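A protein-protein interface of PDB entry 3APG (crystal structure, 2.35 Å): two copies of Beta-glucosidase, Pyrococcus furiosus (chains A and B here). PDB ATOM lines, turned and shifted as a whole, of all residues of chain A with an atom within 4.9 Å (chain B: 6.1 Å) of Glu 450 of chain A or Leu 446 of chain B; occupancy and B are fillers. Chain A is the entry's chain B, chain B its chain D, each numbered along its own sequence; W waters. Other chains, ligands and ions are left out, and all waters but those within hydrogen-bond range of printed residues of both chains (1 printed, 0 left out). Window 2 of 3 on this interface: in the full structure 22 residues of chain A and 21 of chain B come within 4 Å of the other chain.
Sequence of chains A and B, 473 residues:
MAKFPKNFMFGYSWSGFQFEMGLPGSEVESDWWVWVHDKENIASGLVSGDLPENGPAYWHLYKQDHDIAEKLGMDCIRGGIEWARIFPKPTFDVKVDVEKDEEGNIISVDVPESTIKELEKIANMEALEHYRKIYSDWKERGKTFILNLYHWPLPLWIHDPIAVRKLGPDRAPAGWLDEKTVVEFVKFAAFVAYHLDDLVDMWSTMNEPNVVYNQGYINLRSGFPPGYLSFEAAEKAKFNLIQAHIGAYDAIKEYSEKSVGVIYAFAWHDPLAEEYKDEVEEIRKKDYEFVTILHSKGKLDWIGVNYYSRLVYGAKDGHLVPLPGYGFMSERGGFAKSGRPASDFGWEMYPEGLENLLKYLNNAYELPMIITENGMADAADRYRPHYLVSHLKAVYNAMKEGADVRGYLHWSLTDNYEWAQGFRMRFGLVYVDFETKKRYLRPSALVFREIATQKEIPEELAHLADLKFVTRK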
ATOM      1  N   LEU A 446      12.544  -7.057  14.123  1.00  0.00           N
ATOM      2  CA  LEU A 446      13.817  -7.572  14.599  1.00  0.00           C
ATOM      3  C   LEU A 446      13.658  -8.881  15.414  1.00  0.00           C
ATOM      4  O   LEU A 446      14.427  -9.838  15.237  1.00  0.00           O
ATOM      5  CB  LEU A 446      14.550  -6.486  15.388  1.00  0.00           C
ATOM      6  CG  LEU A 446      14.945  -5.310  14.502  1.00  0.00           C
ATOM      7  CD1 LEU A 446      15.690  -4.237  15.297  1.00  0.00           C
ATOM      8  CD2 LEU A 446      15.887  -5.782  13.439  1.00  0.00           C
ATOM      9  N   VAL A 447      12.663  -8.891  16.293  1.00  0.00           N
ATOM     10  CA  VAL A 447      12.304 -10.001  17.144  1.00  0.00           C
ATOM     11  C   VAL A 447      11.852 -11.135  16.229  1.00  0.00           C
ATOM     12  O   VAL A 447      12.359 -12.253  16.321  1.00  0.00           O
ATOM     13  CB  VAL A 447      11.208  -9.525  18.075  1.00  0.00           C
ATOM     14  CG1 VAL A 447      10.671 -10.599  18.875  1.00  0.00           C
ATOM     15  CG2 VAL A 447      11.761  -8.456  18.944  1.00  0.00           C
ATOM     16  N   PHE A 448      10.995 -10.844  15.254  1.00  0.00           N
ATOM     17  CA  PHE A 448      10.565 -11.870  14.331  1.00  0.00           C
ATOM     18  C   PHE A 448      11.808 -12.458  13.675  1.00  0.00           C
ATOM     19  O   PHE A 448      11.946 -13.675  13.517  1.00  0.00           O
ATOM     20  CB  PHE A 448       9.666 -11.262  13.253  1.00  0.00           C
ATOM     21  CG  PHE A 448       8.935 -12.276  12.437  1.00  0.00           C
ATOM     22  CD1 PHE A 448       7.572 -12.494  12.628  1.00  0.00           C
ATOM     23  CD2 PHE A 448       9.594 -13.017  11.494  1.00  0.00           C
ATOM     24  CE1 PHE A 448       6.855 -13.487  11.896  1.00  0.00           C
ATOM     25  CE2 PHE A 448       8.896 -13.989  10.683  1.00  0.00           C
ATOM     26  CZ  PHE A 448       7.557 -14.247  10.898  1.00  0.00           C
ATOM     27  N   ARG A 449      12.747 -11.600  13.274  1.00  0.00           N
ATOM     28  CA  ARG A 449      13.882 -12.124  12.459  1.00  0.00           C
ATOM     29  C   ARG A 449      14.638 -13.138  13.269  1.00  0.00           C
ATOM     30  O   ARG A 449      14.995 -14.232  12.786  1.00  0.00           O
ATOM     31  CB  ARG A 449      14.799 -11.004  12.083  1.00  0.00           C
ATOM     32  CG  ARG A 449      16.135 -11.434  11.530  1.00  0.00           C
ATOM     33  CD  ARG A 449      16.358 -10.548  10.412  1.00  0.00           C
ATOM     34  NE  ARG A 449      16.967  -9.363  10.876  1.00  0.00           N
ATOM     35  CZ  ARG A 449      16.984  -8.192  10.248  1.00  0.00           C
ATOM     36  NH1 ARG A 449      16.360  -7.984   9.069  1.00  0.00           N
ATOM     37  NH2 ARG A 449      17.697  -7.215  10.832  1.00  0.00           N
ATOM     38  N   GLU A 450      14.891 -12.754  14.523  1.00  0.00           N
ATOM     39  CA  GLU A 450      15.671 -13.558  15.385  1.00  0.00           C
ATOM     40  C   GLU A 450      14.962 -14.920  15.610  1.00  0.00           C
ATOM     41  O   GLU A 450      15.596 -15.971  15.520  1.00  0.00           O
ATOM     42  CB  GLU A 450      15.897 -12.851  16.691  1.00  0.00           C
ATOM     43  CG  GLU A 450      16.703 -13.766  17.530  1.00  0.00           C
ATOM     44  CD  GLU A 450      17.473 -13.059  18.596  1.00  0.00           C
ATOM     45  OE1 GLU A 450      17.824 -11.862  18.410  1.00  0.00           O
ATOM     46  OE2 GLU A 450      17.715 -13.726  19.620  1.00  0.00           O
ATOM     47  N   ILE A 451      13.657 -14.891  15.852  1.00  0.00           N
ATOM     48  CA  ILE A 451      12.931 -16.142  16.058  1.00  0.00           C
ATOM     49  C   ILE A 451      12.908 -17.030  14.834  1.00  0.00           C
ATOM     50  O   ILE A 451      13.315 -18.168  14.948  1.00  0.00           O
ATOM     51  CB  ILE A 451      11.489 -15.926  16.601  1.00  0.00           C
ATOM     52  CG1 ILE A 451      11.601 -15.411  18.039  1.00  0.00           C
ATOM     53  CG2 ILE A 451      10.650 -17.200  16.482  1.00  0.00           C
ATOM     54  CD1 ILE A 451      10.331 -15.102  18.732  1.00  0.00           C
ATOM     55  N   ALA A 452      12.479 -16.524  13.681  1.00  0.00           N
ATOM     56  CA  ALA A 452      12.343 -17.344  12.476  1.00  0.00           C
ATOM     57  C   ALA A 452      13.647 -17.880  11.961  1.00  0.00           C
ATOM     58  O   ALA A 452      13.690 -19.003  11.445  1.00  0.00           O
ATOM     59  CB  ALA A 452      11.658 -16.586  11.379  1.00  0.00           C
ATOM     60  N   THR A 453      14.722 -17.124  12.087  1.00  0.00           N
ATOM     61  CA  THR A 453      15.899 -17.623  11.503  1.00  0.00           C
ATOM     62  C   THR A 453      16.458 -18.786  12.327  1.00  0.00           C
ATOM     63  O   THR A 453      16.954 -19.780  11.781  1.00  0.00           O
ATOM     64  CB  THR A 453      16.930 -16.525  11.141  1.00  0.00           C
ATOM     65  OG1 THR A 453      17.346 -15.912  12.306  1.00  0.00           O
ATOM     66  CG2 THR A 453      16.293 -15.431  10.311  1.00  0.00           C
ATOM     67  N   GLN A 454      16.341 -18.711  13.645  1.00  0.00           N
ATOM     68  CA  GLN A 454      16.713 -19.849  14.468  1.00  0.00           C
ATOM     69  C   GLN A 454      15.583 -20.887  14.566  1.00  0.00           C
ATOM     70  O   GLN A 454      15.765 -21.952  15.159  1.00  0.00           O
ATOM     71  CB  GLN A 454      17.106 -19.368  15.878  1.00  0.00           C
ATOM     72  CG  GLN A 454      18.387 -18.486  15.936  1.00  0.00           C
ATOM     73  CD  GLN A 454      18.697 -18.080  17.370  1.00  0.00           C
ATOM     74  OE1 GLN A 454      18.919 -16.903  17.683  1.00  0.00           O
ATOM     75  NE2 GLN A 454      18.702 -19.070  18.264  1.00  0.00           N
ATOM     76  N   GLU A 456      13.243 -20.944  16.625  1.00  0.00           N
ATOM     77  CA  GLU A 456      12.989 -21.211  18.030  1.00  0.00           C
ATOM     78  C   GLU A 456      12.739 -19.884  18.733  1.00  0.00           C
ATOM     79  O   GLU A 456      13.128 -18.829  18.213  1.00  0.00           O
ATOM     80  CB  GLU A 456      14.168 -21.971  18.680  1.00  0.00           C
ATOM     81  CG  GLU A 456      15.360 -21.100  19.029  1.00  0.00           C
ATOM     82  CD  GLU A 456      16.504 -21.798  19.801  1.00  0.00           C
ATOM     83  OE1 GLU A 456      16.321 -22.495  20.834  1.00  0.00           O
ATOM     84  OE2 GLU A 456      17.656 -21.565  19.409  1.00  0.00           O
ATOM     85  N   PRO A 458      14.287 -18.166  21.420  1.00  0.00           N
ATOM     86  CA  PRO A 458      15.501 -18.351  22.213  1.00  0.00           C
ATOM     87  C   PRO A 458      15.345 -17.878  23.637  1.00  0.00           C
ATOM     88  O   PRO A 458      14.508 -17.051  23.922  1.00  0.00           O
ATOM     89  CB  PRO A 458      16.535 -17.497  21.475  1.00  0.00           C
ATOM     90  CG  PRO A 458      15.750 -16.565  20.630  1.00  0.00           C
ATOM     91  CD  PRO A 458      14.408 -17.125  20.384  1.00  0.00           C
ATOM     92  N   GLU A 460      17.051 -15.682  25.439  1.00  0.00           N
ATOM     93  CA  GLU A 460      17.145 -14.242  25.631  1.00  0.00           C
ATOM     94  C   GLU A 460      15.855 -13.526  25.214  1.00  0.00           C
ATOM     95  O   GLU A 460      15.646 -12.358  25.549  1.00  0.00           O
ATOM     96  CB  GLU A 460      18.335 -13.702  24.873  1.00  0.00           C
ATOM     97  CG  GLU A 460      18.170 -13.748  23.387  1.00  0.00           C
ATOM     98  CD  GLU A 460      19.401 -13.282  22.600  1.00  0.00           C
ATOM     99  OE1 GLU A 460      20.459 -12.984  23.221  1.00  0.00           O
ATOM    100  OE2 GLU A 460      19.311 -13.204  21.333  1.00  0.00           O
ATOM    101  N   LEU A 461      14.984 -14.199  24.473  1.00  0.00           N
ATOM    102  CA  LEU A 461      13.710 -13.561  24.130  1.00  0.00           C
ATOM    103  C   LEU A 461      12.473 -14.206  24.823  1.00  0.00           C
ATOM    104  O   LEU A 461      11.338 -13.785  24.598  1.00  0.00           O
ATOM    105  CB  LEU A 461      13.489 -13.449  22.600  1.00  0.00           C
ATOM    106  CG  LEU A 461      14.556 -12.754  21.746  1.00  0.00           C
ATOM    107  CD1 LEU A 461      14.101 -12.751  20.342  1.00  0.00           C
ATOM    108  CD2 LEU A 461      14.831 -11.323  22.126  1.00  0.00           C
ATOM    109  N   LEU B  72      26.231  -5.817  22.105  1.00  0.00           N
ATOM    110  CA  LEU B  72      25.340  -4.790  21.594  1.00  0.00           C
ATOM    111  C   LEU B  72      26.148  -3.617  20.935  1.00  0.00           C
ATOM    112  O   LEU B  72      25.592  -2.548  20.664  1.00  0.00           O
ATOM    113  CB  LEU B  72      24.492  -4.201  22.713  1.00  0.00           C
ATOM    114  CG  LEU B  72      23.650  -5.056  23.650  1.00  0.00           C
ATOM    115  CD1 LEU B  72      23.221  -4.260  24.864  1.00  0.00           C
ATOM    116  CD2 LEU B  72      22.439  -5.734  22.903  1.00  0.00           C
ATOM    117  N   LEU B 441      16.967 -10.007  26.908  1.00  0.00           N
ATOM    118  CA  LEU B 441      17.012  -8.848  26.001  1.00  0.00           C
ATOM    119  C   LEU B 441      15.636  -8.251  25.851  1.00  0.00           C
ATOM    120  O   LEU B 441      14.624  -8.986  25.848  1.00  0.00           O
ATOM    121  CB  LEU B 441      17.515  -9.268  24.636  1.00  0.00           C
ATOM    122  CG  LEU B 441      19.012  -9.559  24.581  1.00  0.00           C
ATOM    123  CD1 LEU B 441      19.458  -9.692  23.140  1.00  0.00           C
ATOM    124  CD2 LEU B 441      19.846  -8.490  25.281  1.00  0.00           C
ATOM    125  N   ARG B 442      15.569  -6.938  25.767  1.00  0.00           N
ATOM    126  CA  ARG B 442      14.363  -6.255  25.337  1.00  0.00           C
ATOM    127  C   ARG B 442      14.642  -5.838  23.878  1.00  0.00           C
ATOM    128  O   ARG B 442      15.803  -5.610  23.520  1.00  0.00           O
ATOM    129  CB  ARG B 442      14.101  -5.038  26.197  1.00  0.00           C
ATOM    130  CG  ARG B 442      13.699  -5.346  27.701  1.00  0.00           C
ATOM    131  CD  ARG B 442      13.087  -4.126  28.452  1.00  0.00           C
ATOM    132  NE  ARG B 442      12.538  -4.505  29.758  1.00  0.00           N
ATOM    133  CZ  ARG B 442      13.102  -4.215  30.942  1.00  0.00           C
ATOM    134  NH1 ARG B 442      14.200  -3.432  31.033  1.00  0.00           N
ATOM    135  NH2 ARG B 442      12.540  -4.666  32.040  1.00  0.00           N
ATOM    136  N   PRO B 443      13.591  -5.705  23.052  1.00  0.00           N
ATOM    137  CA  PRO B 443      13.742  -5.272  21.678  1.00  0.00           C
ATOM    138  C   PRO B 443      14.560  -3.983  21.552  1.00  0.00           C
ATOM    139  O   PRO B 443      15.345  -3.834  20.589  1.00  0.00           O
ATOM    140  CB  PRO B 443      12.300  -5.009  21.227  1.00  0.00           C
ATOM    141  CG  PRO B 443      11.509  -5.882  22.047  1.00  0.00           C
ATOM    142  CD  PRO B 443      12.175  -5.930  23.401  1.00  0.00           C
ATOM    143  N   SER B 444      14.410  -3.065  22.502  1.00  0.00           N
ATOM    144  CA  SER B 444      15.288  -1.899  22.472  1.00  0.00           C
ATOM    145  C   SER B 444      16.755  -2.275  22.465  1.00  0.00           C
ATOM    146  O   SER B 444      17.573  -1.525  21.948  1.00  0.00           O
ATOM    147  CB  SER B 444      15.005  -0.908  23.610  1.00  0.00           C
ATOM    148  OG  SER B 444      14.919  -1.561  24.866  1.00  0.00           O
ATOM    149  N   ALA B 445      17.118  -3.430  23.030  1.00  0.00           N
ATOM    150  CA  ALA B 445      18.543  -3.805  23.004  1.00  0.00           C
ATOM    151  C   ALA B 445      18.926  -4.118  21.527  1.00  0.00           C
ATOM    152  O   ALA B 445      20.056  -3.762  21.065  1.00  0.00           O
ATOM    153  CB  ALA B 445      18.774  -4.961  23.876  1.00  0.00           C
ATOM    154  N   LEU B 446      18.002  -4.761  20.796  1.00  0.00           N
ATOM    155  CA  LEU B 446      18.253  -5.086  19.398  1.00  0.00           C
ATOM    156  C   LEU B 446      18.378  -3.805  18.568  1.00  0.00           C
ATOM    157  O   LEU B 446      19.217  -3.710  17.664  1.00  0.00           O
ATOM    158  CB  LEU B 446      17.177  -5.975  18.801  1.00  0.00           C
ATOM    159  CG  LEU B 446      16.936  -7.369  19.451  1.00  0.00           C
ATOM    160  CD1 LEU B 446      15.718  -8.024  18.763  1.00  0.00           C
ATOM    161  CD2 LEU B 446      18.146  -8.352  19.454  1.00  0.00           C
ATOM    162  N   VAL B 447      17.565  -2.810  18.877  1.00  0.00           N
ATOM    163  CA  VAL B 447      17.703  -1.526  18.216  1.00  0.00           C
ATOM    164  C   VAL B 447      19.080  -0.905  18.561  1.00  0.00           C
ATOM    165  O   VAL B 447      19.812  -0.490  17.706  1.00  0.00           O
ATOM    166  CB  VAL B 447      16.480  -0.587  18.591  1.00  0.00           C
ATOM    167  CG1 VAL B 447      16.689   0.835  18.067  1.00  0.00           C
ATOM    168  CG2 VAL B 447      15.189  -1.144  18.039  1.00  0.00           C
ATOM    169  N   PHE B 448      19.423  -0.871  19.838  1.00  0.00           N
ATOM    170  CA  PHE B 448      20.722  -0.350  20.293  1.00  0.00           C
ATOM    171  C   PHE B 448      21.911  -1.053  19.567  1.00  0.00           C
ATOM    172  O   PHE B 448      22.768  -0.373  18.939  1.00  0.00           O
ATOM    173  CB  PHE B 448      20.813  -0.392  21.818  1.00  0.00           C
ATOM    174  CG  PHE B 448      21.969   0.406  22.377  1.00  0.00           C
ATOM    175  CD1 PHE B 448      21.744   1.521  23.152  1.00  0.00           C
ATOM    176  CD2 PHE B 448      23.304   0.044  22.095  1.00  0.00           C
ATOM    177  CE1 PHE B 448      22.837   2.255  23.638  1.00  0.00           C
ATOM    178  CE2 PHE B 448      24.371   0.760  22.576  1.00  0.00           C
ATOM    179  CZ  PHE B 448      24.159   1.858  23.339  1.00  0.00           C
ATOM    180  N   ARG B 449      21.880  -2.394  19.527  1.00  0.00           N
ATOM    181  CA  ARG B 449      22.895  -3.168  18.828  1.00  0.00           C
ATOM    182  C   ARG B 449      23.005  -2.711  17.393  1.00  0.00           C
ATOM    183  O   ARG B 449      24.116  -2.607  16.854  1.00  0.00           O
ATOM    184  CB  ARG B 449      22.524  -4.631  18.815  1.00  0.00           C
ATOM    185  CG  ARG B 449      23.413  -5.608  17.964  1.00  0.00           C
ATOM    186  CD  ARG B 449      23.623  -6.814  18.834  1.00  0.00           C
ATOM    187  NE  ARG B 449      22.581  -7.841  18.702  1.00  0.00           N
ATOM    188  CZ  ARG B 449      22.316  -8.796  19.623  1.00  0.00           C
ATOM    189  NH1 ARG B 449      22.961  -8.852  20.811  1.00  0.00           N
ATOM    190  NH2 ARG B 449      21.383  -9.714  19.354  1.00  0.00           N
ATOM    191  N   GLU B 450      21.875  -2.499  16.741  1.00  0.00           N
ATOM    192  CA  GLU B 450      21.959  -2.221  15.317  1.00  0.00           C
ATOM    193  C   GLU B 450      22.553  -0.832  15.098  1.00  0.00           C
ATOM    194  O   GLU B 450      23.324  -0.630  14.194  1.00  0.00           O
ATOM    195  CB  GLU B 450      20.626  -2.337  14.619  1.00  0.00           C
ATOM    196  CG  GLU B 450      20.779  -1.925  13.190  1.00  0.00           C
ATOM    197  CD  GLU B 450      19.589  -2.281  12.341  1.00  0.00           C
ATOM    198  OE1 GLU B 450      18.920  -3.286  12.672  1.00  0.00           O
ATOM    199  OE2 GLU B 450      19.314  -1.544  11.361  1.00  0.00           O
ATOM    200  N   ILE B 451      22.207   0.119  15.965  1.00  0.00           N
ATOM    201  CA  ILE B 451      22.633   1.490  15.777  1.00  0.00           C
ATOM    202  C   ILE B 451      24.109   1.651  16.140  1.00  0.00           C
ATOM    203  O   ILE B 451      24.872   2.203  15.367  1.00  0.00           O
ATOM    204  CB  ILE B 451      21.793   2.393  16.631  1.00  0.00           C
ATOM    205  CG1 ILE B 451      20.383   2.529  16.036  1.00  0.00           C
ATOM    206  CG2 ILE B 451      22.420   3.781  16.742  1.00  0.00           C
ATOM    207  CD1 ILE B 451      19.493   3.343  16.899  1.00  0.00           C
ATOM    208  N   LEU B 461      15.585   2.236  10.420  1.00  0.00           N
ATOM    209  CA  LEU B 461      15.217   2.542  11.803  1.00  0.00           C
ATOM    210  C   LEU B 461      14.962   4.027  12.091  1.00  0.00           C
ATOM    211  O   LEU B 461      14.791   4.406  13.257  1.00  0.00           O
ATOM    212  CB  LEU B 461      16.268   2.068  12.837  1.00  0.00           C
ATOM    213  CG  LEU B 461      16.541   0.559  12.919  1.00  0.00           C
ATOM    214  CD1 LEU B 461      17.362   0.314  14.116  1.00  0.00           C
ATOM    215  CD2 LEU B 461      15.294  -0.265  13.014  1.00  0.00           C
HETATM  216  O   HOH W   1      13.044 -11.653  26.970  1.00  0.00           O
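The backbone carbonyl oxygen (O) of Glu 460 of chain A sits at hydrogen-bond distance from the backbone NH (N) of Leu 441 of chain B (3.0 Å).
Among the printed residues, pairs that only touch across the chains: Leu 446 of chain A with Leu 446 of chain B (3.9 Å), Val 447 of chain A with Leu 446 of chain B (3.98 Å) and Glu 450 of chain A with Leu 446 of chain B (3.7 Å).
Of the printed residues of chain B, Glu 450 of chain A touches Leu 446 (3.7 Å). Of the printed residues of chain A, Leu 446 of chain B touches Leu 446, Val 447 and Glu 450. Of the printed residues of chain B, Glu 460 of chain A touches Leu 441. Of the printed residues of chain B, Val 447 of chain A touches Leu 446 (3.98 Å). Of the printed residues of chain A, Leu 441 of chain B touches Glu 460 (3.0 Å). Ile 451 of chain B touches none of the printed residues of chain A. The nearest residue of chain B that does not touch Glu 450 of chain A is Arg 449 of chain B (4.3 Å). The nearest printed residue of chain B that does not touch Glu 460 of chain A is Arg 449 of chain B (4.5 Å).
Of the 13 printed residues of chain B, 2 touch a printed residue of chain A. Among the printed residues, 4 pairs touch across the chains. Among the printed residues, no Asp or Glu carboxylate lies within 4 Å of a Lys or Arg side-chain nitrogen of the other chain.
Leu 446 of chain B touches its own counterpart, Leu 446 of chain A. Val 447 of chain A touches Leu 446 of chain B, but with the chains exchanged Leu 446 of chain A does not touch Val 447 of chain B (4.2 Å). Glu 450 of chain A touches Leu 446 of chain B, but with the chains exchanged Leu 446 of chain A does not touch Glu 450 of chain B (4.002 Å).
Water W1 bridges the backbone carbonyl oxygen of Glu 460 of chain A (3.0 Å) and the backbone carbonyl oxygen of Leu 441 of chain B (3.3 Å).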
